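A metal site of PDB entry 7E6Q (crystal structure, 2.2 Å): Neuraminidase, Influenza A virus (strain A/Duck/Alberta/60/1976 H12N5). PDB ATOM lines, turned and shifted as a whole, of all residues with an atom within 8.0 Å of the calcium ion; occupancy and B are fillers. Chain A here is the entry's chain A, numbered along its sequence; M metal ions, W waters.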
ATOM      1  N   HIS A 194     -23.734   3.993  33.896  1.00  0.00           N
ATOM      2  CA  HIS A 194     -24.080   5.365  34.272  1.00  0.00           C
ATOM      3  C   HIS A 194     -25.381   5.364  35.053  1.00  0.00           C
ATOM      4  O   HIS A 194     -26.356   4.759  34.612  1.00  0.00           O
ATOM      5  CB  HIS A 194     -24.214   6.246  33.019  1.00  0.00           C
ATOM      6  CG  HIS A 194     -24.027   7.704  33.284  1.00  0.00           C
ATOM      7  ND1 HIS A 194     -25.049   8.623  33.159  1.00  0.00           N
ATOM      8  CD2 HIS A 194     -22.933   8.398  33.667  1.00  0.00           C
ATOM      9  CE1 HIS A 194     -24.588   9.823  33.452  1.00  0.00           C
ATOM     10  NE2 HIS A 194     -23.304   9.718  33.763  1.00  0.00           N
ATOM     11  N   ARG A 212     -31.588   5.815  35.401  1.00  0.00           N
ATOM     12  CA  ARG A 212     -31.420   6.334  34.033  1.00  0.00           C
ATOM     13  C   ARG A 212     -29.933   6.374  33.686  1.00  0.00           C
ATOM     14  O   ARG A 212     -29.120   6.880  34.479  1.00  0.00           O
ATOM     15  CB  ARG A 212     -32.086   7.703  33.914  1.00  0.00           C
ATOM     16  CG  ARG A 212     -31.467   8.650  32.902  1.00  0.00           C
ATOM     17  CD  ARG A 212     -31.984  10.059  33.028  1.00  0.00           C
ATOM     18  NE  ARG A 212     -31.468  10.979  32.045  1.00  0.00           N
ATOM     19  CZ  ARG A 212     -31.909  12.209  31.869  1.00  0.00           C
ATOM     20  NH1 ARG A 212     -32.871  12.668  32.627  1.00  0.00           N
ATOM     21  NH2 ARG A 212     -31.409  12.972  30.942  1.00  0.00           N
ATOM     22  N   ASP A 213     -29.613   5.823  32.542  1.00  0.00           N
ATOM     23  CA  ASP A 213     -28.265   5.857  31.974  1.00  0.00           C
ATOM     24  C   ASP A 213     -28.207   7.032  30.999  1.00  0.00           C
ATOM     25  O   ASP A 213     -28.828   6.994  29.935  1.00  0.00           O
ATOM     26  CB  ASP A 213     -27.935   4.543  31.278  1.00  0.00           C
ATOM     27  CG  ASP A 213     -26.515   4.497  30.712  1.00  0.00           C
ATOM     28  OD1 ASP A 213     -26.110   5.427  29.990  1.00  0.00           O
ATOM     29  OD2 ASP A 213     -25.817   3.494  30.975  1.00  0.00           O
ATOM     30  N   ASN A 214     -27.430   8.058  31.348  1.00  0.00           N
ATOM     31  CA  ASN A 214     -27.265   9.232  30.497  1.00  0.00           C
ATOM     32  C   ASN A 214     -25.989   9.163  29.649  1.00  0.00           C
ATOM     33  O   ASN A 214     -25.553  10.195  29.131  1.00  0.00           O
ATOM     34  CB  ASN A 214     -27.258  10.494  31.356  1.00  0.00           C
ATOM     35  CG  ASN A 214     -27.929  11.673  30.661  1.00  0.00           C
ATOM     36  OD1 ASN A 214     -29.051  11.566  30.175  1.00  0.00           O
ATOM     37  ND2 ASN A 214     -27.241  12.810  30.628  1.00  0.00           N
ATOM     38  N   TRP A 215     -25.368   7.975  29.528  1.00  0.00           N
ATOM     39  CA  TRP A 215     -24.103   7.865  28.800  1.00  0.00           C
ATOM     40  C   TRP A 215     -24.158   6.928  27.586  1.00  0.00           C
ATOM     41  O   TRP A 215     -24.192   7.424  26.453  1.00  0.00           O
ATOM     42  CB  TRP A 215     -23.053   7.401  29.806  1.00  0.00           C
ATOM     43  CG  TRP A 215     -21.659   7.300  29.286  1.00  0.00           C
ATOM     44  CD1 TRP A 215     -21.163   7.874  28.163  1.00  0.00           C
ATOM     45  CD2 TRP A 215     -20.589   6.548  29.868  1.00  0.00           C
ATOM     46  NE1 TRP A 215     -19.830   7.546  28.012  1.00  0.00           N
ATOM     47  CE2 TRP A 215     -19.462   6.728  29.048  1.00  0.00           C
ATOM     48  CE3 TRP A 215     -20.477   5.752  31.010  1.00  0.00           C
ATOM     49  CZ2 TRP A 215     -18.231   6.133  29.334  1.00  0.00           C
ATOM     50  CZ3 TRP A 215     -19.260   5.159  31.298  1.00  0.00           C
ATOM     51  CH2 TRP A 215     -18.150   5.350  30.448  1.00  0.00           C
ATOM     52  N   ASN A 216     -24.266   5.618  27.776  1.00  0.00           N
ATOM     53  CA  ASN A 216     -24.163   4.651  26.677  1.00  0.00           C
ATOM     54  C   ASN A 216     -25.238   3.587  26.754  1.00  0.00           C
ATOM     55  O   ASN A 216     -25.083   2.508  26.175  1.00  0.00           O
ATOM     56  CB  ASN A 216     -22.783   3.968  26.631  1.00  0.00           C
ATOM     57  CG  ASN A 216     -21.668   4.903  26.190  1.00  0.00           C
ATOM     58  OD1 ASN A 216     -21.832   5.721  25.293  1.00  0.00           O
ATOM     59  ND2 ASN A 216     -20.503   4.755  26.821  1.00  0.00           N
ATOM     60  N   GLY A 217     -26.335   3.846  27.471  1.00  0.00           N
ATOM     61  CA  GLY A 217     -27.349   2.838  27.629  1.00  0.00           C
ATOM     62  C   GLY A 217     -28.747   3.343  27.374  1.00  0.00           C
ATOM     63  O   GLY A 217     -29.180   4.339  27.965  1.00  0.00           O
ATOM     64  N   MET A 218     -29.444   2.687  26.452  1.00  0.00           N
ATOM     65  CA  MET A 218     -30.872   2.872  26.279  1.00  0.00           C
ATOM     66  C   MET A 218     -31.677   1.874  27.101  1.00  0.00           C
ATOM     67  O   MET A 218     -32.909   1.949  27.108  1.00  0.00           O
ATOM     68  CB  MET A 218     -31.247   2.758  24.790  1.00  0.00           C
ATOM     69  CG  MET A 218     -31.300   1.343  24.256  1.00  0.00           C
ATOM     70  SD  MET A 218     -31.663   1.293  22.488  1.00  0.00           S
ATOM     71  CE  MET A 218     -30.033   1.607  21.808  1.00  0.00           C
ATOM     72  N   ASN A 219     -31.009   0.945  27.773  1.00  0.00           N
ATOM     73  CA  ASN A 219     -31.595   0.172  28.857  1.00  0.00           C
ATOM     74  C   ASN A 219     -31.251   0.815  30.198  1.00  0.00           C
ATOM     75  O   ASN A 219     -30.318   1.602  30.325  1.00  0.00           O
ATOM     76  CB  ASN A 219     -31.128  -1.293  28.814  1.00  0.00           C
ATOM     77  CG  ASN A 219     -29.612  -1.432  28.745  1.00  0.00           C
ATOM     78  OD1 ASN A 219     -28.878  -0.445  28.685  1.00  0.00           O
ATOM     79  ND2 ASN A 219     -29.148  -2.669  28.802  1.00  0.00           N
ATOM     80  N   ARG A 220     -32.055   0.462  31.213  1.00  0.00           N
ATOM     81  CA  ARG A 220     -32.008   1.174  32.482  1.00  0.00           C
ATOM     82  C   ARG A 220     -31.176   0.420  33.504  1.00  0.00           C
ATOM     83  O   ARG A 220     -31.358  -0.803  33.660  1.00  0.00           O
ATOM     84  CB  ARG A 220     -33.427   1.380  33.032  1.00  0.00           C
ATOM     85  CG  ARG A 220     -34.283   2.283  32.175  1.00  0.00           C
ATOM     86  CD  ARG A 220     -35.469   2.794  32.973  1.00  0.00           C
ATOM     87  NE  ARG A 220     -36.257   3.769  32.221  1.00  0.00           N
ATOM     88  CZ  ARG A 220     -35.932   5.055  32.101  1.00  0.00           C
ATOM     89  NH1 ARG A 220     -34.839   5.526  32.679  1.00  0.00           N
ATOM     90  NH2 ARG A 220     -36.722   5.870  31.403  1.00  0.00           N
ATOM     91  N   PRO A 221     -30.283   1.100  34.205  1.00  0.00           N
ATOM     92  CA  PRO A 221     -29.525   0.442  35.276  1.00  0.00           C
ATOM     93  C   PRO A 221     -30.435  -0.022  36.408  1.00  0.00           C
ATOM     94  O   PRO A 221     -31.462   0.587  36.700  1.00  0.00           O
ATOM     95  CB  PRO A 221     -28.565   1.545  35.759  1.00  0.00           C
ATOM     96  CG  PRO A 221     -28.499   2.522  34.631  1.00  0.00           C
ATOM     97  CD  PRO A 221     -29.861   2.492  34.002  1.00  0.00           C
ATOM     98  N   TYR A 235     -28.088  -3.910  34.763  1.00  0.00           N
ATOM     99  CA  TYR A 235     -29.099  -3.306  33.916  1.00  0.00           C
ATOM    100  C   TYR A 235     -30.331  -4.198  33.885  1.00  0.00           C
ATOM    101  O   TYR A 235     -30.265  -5.387  34.181  1.00  0.00           O
ATOM    102  CB  TYR A 235     -28.586  -3.058  32.491  1.00  0.00           C
ATOM    103  CG  TYR A 235     -27.632  -1.892  32.392  1.00  0.00           C
ATOM    104  CD1 TYR A 235     -26.333  -1.998  32.853  1.00  0.00           C
ATOM    105  CD2 TYR A 235     -28.027  -0.697  31.811  1.00  0.00           C
ATOM    106  CE1 TYR A 235     -25.450  -0.929  32.755  1.00  0.00           C
ATOM    107  CE2 TYR A 235     -27.158   0.375  31.715  1.00  0.00           C
ATOM    108  CZ  TYR A 235     -25.872   0.259  32.193  1.00  0.00           C
ATOM    109  OH  TYR A 235     -25.011   1.326  32.094  1.00  0.00           O
ATOM    110  N   ASP A 243     -35.644   3.309  28.143  1.00  0.00           N
ATOM    111  CA  ASP A 243     -35.206   4.691  28.198  1.00  0.00           C
ATOM    112  C   ASP A 243     -35.744   5.454  26.993  1.00  0.00           C
ATOM    113  O   ASP A 243     -36.361   4.886  26.088  1.00  0.00           O
ATOM    114  CB  ASP A 243     -33.674   4.765  28.230  1.00  0.00           C
ATOM    115  CG  ASP A 243     -33.155   6.082  28.790  1.00  0.00           C
ATOM    116  OD1 ASP A 243     -33.957   7.018  28.968  1.00  0.00           O
ATOM    117  OD2 ASP A 243     -31.934   6.174  29.050  1.00  0.00           O
ATOM    118  N   THR A 244     -35.520   6.764  26.992  1.00  0.00           N
ATOM    119  CA  THR A 244     -35.791   7.611  25.840  1.00  0.00           C
ATOM    120  C   THR A 244     -34.638   8.601  25.706  1.00  0.00           C
ATOM    121  O   THR A 244     -34.345   9.323  26.667  1.00  0.00           O
ATOM    122  CB  THR A 244     -37.124   8.358  25.999  1.00  0.00           C
ATOM    123  OG1 THR A 244     -38.165   7.434  26.347  1.00  0.00           O
ATOM    124  CG2 THR A 244     -37.499   9.059  24.709  1.00  0.00           C
ATOM    125  N   PRO A 245     -33.974   8.668  24.546  1.00  0.00           N
ATOM    126  CA  PRO A 245     -34.265   7.971  23.289  1.00  0.00           C
ATOM    127  C   PRO A 245     -33.875   6.491  23.286  1.00  0.00           C
ATOM    128  O   PRO A 245     -33.129   6.035  24.159  1.00  0.00           O
ATOM    129  CB  PRO A 245     -33.438   8.733  22.261  1.00  0.00           C
ATOM    130  CG  PRO A 245     -32.299   9.277  23.034  1.00  0.00           C
ATOM    131  CD  PRO A 245     -32.816   9.581  24.403  1.00  0.00           C
ATOM    132  N   ARG A 246     -34.399   5.758  22.305  1.00  0.00           N
ATOM    133  CA  ARG A 246     -34.090   4.341  22.122  1.00  0.00           C
ATOM    134  C   ARG A 246     -34.364   3.982  20.671  1.00  0.00           C
ATOM    135  O   ARG A 246     -34.718   4.843  19.857  1.00  0.00           O
ATOM    136  CB  ARG A 246     -34.895   3.476  23.096  1.00  0.00           C
ATOM    137  CG  ARG A 246     -36.411   3.660  22.973  1.00  0.00           C
ATOM    138  CD  ARG A 246     -37.165   2.714  23.910  1.00  0.00           C
ATOM    139  NE  ARG A 246     -38.609   2.681  23.645  1.00  0.00           N
ATOM    140  CZ  ARG A 246     -39.462   3.667  23.900  1.00  0.00           C
ATOM    141  NH1 ARG A 246     -39.049   4.800  24.444  1.00  0.00           N
ATOM    142  NH2 ARG A 246     -40.746   3.512  23.604  1.00  0.00           N
ATOM    143  N   VAL A 260     -26.386  -1.066  26.591  1.00  0.00           N
ATOM    144  CA  VAL A 260     -26.553  -1.235  25.147  1.00  0.00           C
ATOM    145  C   VAL A 260     -27.055   0.093  24.593  1.00  0.00           C
ATOM    146  O   VAL A 260     -28.080   0.620  25.049  1.00  0.00           O
ATOM    147  CB  VAL A 260     -27.545  -2.365  24.820  1.00  0.00           C
ATOM    148  CG1 VAL A 260     -27.632  -2.592  23.319  1.00  0.00           C
ATOM    149  CG2 VAL A 260     -27.125  -3.645  25.537  1.00  0.00           C
ATOM    150  N   GLY A 261     -26.345   0.642  23.614  1.00  0.00           N
ATOM    151  CA  GLY A 261     -26.625   1.982  23.107  1.00  0.00           C
ATOM    152  C   GLY A 261     -26.338   2.125  21.639  1.00  0.00           C
ATOM    153  O   GLY A 261     -26.614   1.206  20.855  1.00  0.00           O
ATOM    154  N   THR A 265     -28.637   7.232  20.246  1.00  0.00           N
ATOM    155  CA  THR A 265     -29.345   7.324  21.516  1.00  0.00           C
ATOM    156  C   THR A 265     -28.439   7.635  22.690  1.00  0.00           C
ATOM    157  O   THR A 265     -28.918   7.659  23.832  1.00  0.00           O
ATOM    158  CB  THR A 265     -30.106   6.013  21.781  1.00  0.00           C
ATOM    159  OG1 THR A 265     -29.162   4.981  22.110  1.00  0.00           O
ATOM    160  CG2 THR A 265     -30.883   5.599  20.541  1.00  0.00           C
ATOM    161  N   ASN A 266     -27.152   7.891  22.458  1.00  0.00           N
ATOM    162  CA  ASN A 266     -26.209   8.091  23.546  1.00  0.00           C
ATOM    163  C   ASN A 266     -26.286   9.510  24.084  1.00  0.00           C
ATOM    164  O   ASN A 266     -26.784  10.427  23.440  1.00  0.00           O
ATOM    165  CB  ASN A 266     -24.783   7.781  23.080  1.00  0.00           C
ATOM    166  CG  ASN A 266     -24.564   6.316  22.759  1.00  0.00           C
ATOM    167  OD1 ASN A 266     -25.234   5.439  23.308  1.00  0.00           O
ATOM    168  ND2 ASN A 266     -23.620   6.041  21.878  1.00  0.00           N
ATOM    169  N   ASN A 267     -25.773   9.678  25.311  1.00  0.00           N
ATOM    170  CA  ASN A 267     -25.624  10.975  25.958  1.00  0.00           C
ATOM    171  C   ASN A 267     -26.964  11.637  26.278  1.00  0.00           C
ATOM    172  O   ASN A 267     -27.055  12.864  26.327  1.00  0.00           O
ATOM    173  CB  ASN A 267     -24.757  11.925  25.124  1.00  0.00           C
ATOM    174  CG  ASN A 267     -23.377  11.343  24.815  1.00  0.00           C
ATOM    175  OD1 ASN A 267     -22.841  10.545  25.588  1.00  0.00           O
ATOM    176  ND2 ASN A 267     -22.809  11.743  23.684  1.00  0.00           N
ATOM    177  N   TYR A 268     -28.014  10.848  26.478  1.00  0.00           N
ATOM    178  CA  TYR A 268     -29.283  11.384  26.954  1.00  0.00           C
ATOM    179  C   TYR A 268     -30.088  10.267  27.609  1.00  0.00           C
ATOM    180  O   TYR A 268     -29.644   9.122  27.698  1.00  0.00           O
ATOM    181  CB  TYR A 268     -30.083  12.053  25.828  1.00  0.00           C
ATOM    182  CG  TYR A 268     -30.989  13.161  26.329  1.00  0.00           C
ATOM    183  CD1 TYR A 268     -30.467  14.262  27.000  1.00  0.00           C
ATOM    184  CD2 TYR A 268     -32.368  13.094  26.151  1.00  0.00           C
ATOM    185  CE1 TYR A 268     -31.290  15.266  27.471  1.00  0.00           C
ATOM    186  CE2 TYR A 268     -33.204  14.101  26.624  1.00  0.00           C
ATOM    187  CZ  TYR A 268     -32.650  15.189  27.285  1.00  0.00           C
ATOM    188  OH  TYR A 268     -33.468  16.186  27.750  1.00  0.00           O
ATOM    189  N   GLY A 269     -31.287  10.618  28.069  1.00  0.00           N
ATOM    190  CA  GLY A 269     -32.149   9.689  28.766  1.00  0.00           C
ATOM    191  C   GLY A 269     -33.355  10.423  29.332  1.00  0.00           C
ATOM    192  O   GLY A 269     -33.546  11.619  29.117  1.00  0.00           O
ATOM    193  N   VAL A 270     -34.182   9.651  30.050  1.00  0.00           N
ATOM    194  CA  VAL A 270     -35.292  10.188  30.829  1.00  0.00           C
ATOM    195  C   VAL A 270     -35.377   9.411  32.137  1.00  0.00           C
ATOM    196  O   VAL A 270     -35.146   8.199  32.163  1.00  0.00           O
ATOM    197  CB  VAL A 270     -36.657  10.114  30.103  1.00  0.00           C
ATOM    198  CG1 VAL A 270     -36.698  11.038  28.922  1.00  0.00           C
ATOM    199  CG2 VAL A 270     -36.965   8.684  29.684  1.00  0.00           C
HETATM  200 CA    CA M   1     -29.761   6.718  27.853  1.00  0.00          CA
HETATM  201  O   HOH W   1     -27.905   7.161  26.503  1.00  0.00           O
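The side-chain carboxylate (OD1) of Asp 213 is in hydrogen-bond range of the backbone NH (N) of Asn 216 (2.9 Å).
OD2 of Asp 213 lies within hydrogen-bond range of OH of Tyr 235.
The guanidinium group of Arg 246 is in hydrogen-bond range of the backbone carbonyl oxygen of Asp 243 (3.2 Å).
The side-chain carboxylate of Asp 213 sits at hydrogen-bond distance from the backbone NH of Gly 217 (3.0 Å).
The side-chain carboxylate (OD1) of Asp 243 lies within hydrogen-bond range of the backbone NH (N) of Val 270, 2.9 Å away.
The side-chain amide oxygen of Asn 214 lies within hydrogen-bond range of the backbone NH of Gly 269, 3.2 Å away.
The backbone carbonyl oxygen of Met 218 sits close to the backbone NH of Asp 243 (3.2 Å).
The side-chain carboxylate (OD1) of Asp 213 is in hydrogen-bond range of the backbone NH (N) of Trp 215.
Merely in contact with the calcium ion: Gly 269 (3.9 Å).
Of the 24 residues printed, 5 come within 4 Å of the calcium ion.
The nearest printed residue that does not touch the calcium ion is Thr 265 (4.2 Å).
The calcium ion is bound by the backbone carbonyl oxygen of Asp 213 (2.3 Å), water W1 (2.3 Å), the backbone carbonyl oxygen of Tyr 268 (2.4 Å), the backbone carbonyl oxygen of Gly 217 (2.5 Å) and the side-chain carboxylate of Asp 243 (2.5 Å).
The calcium ion has five donor atoms within binding distance.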
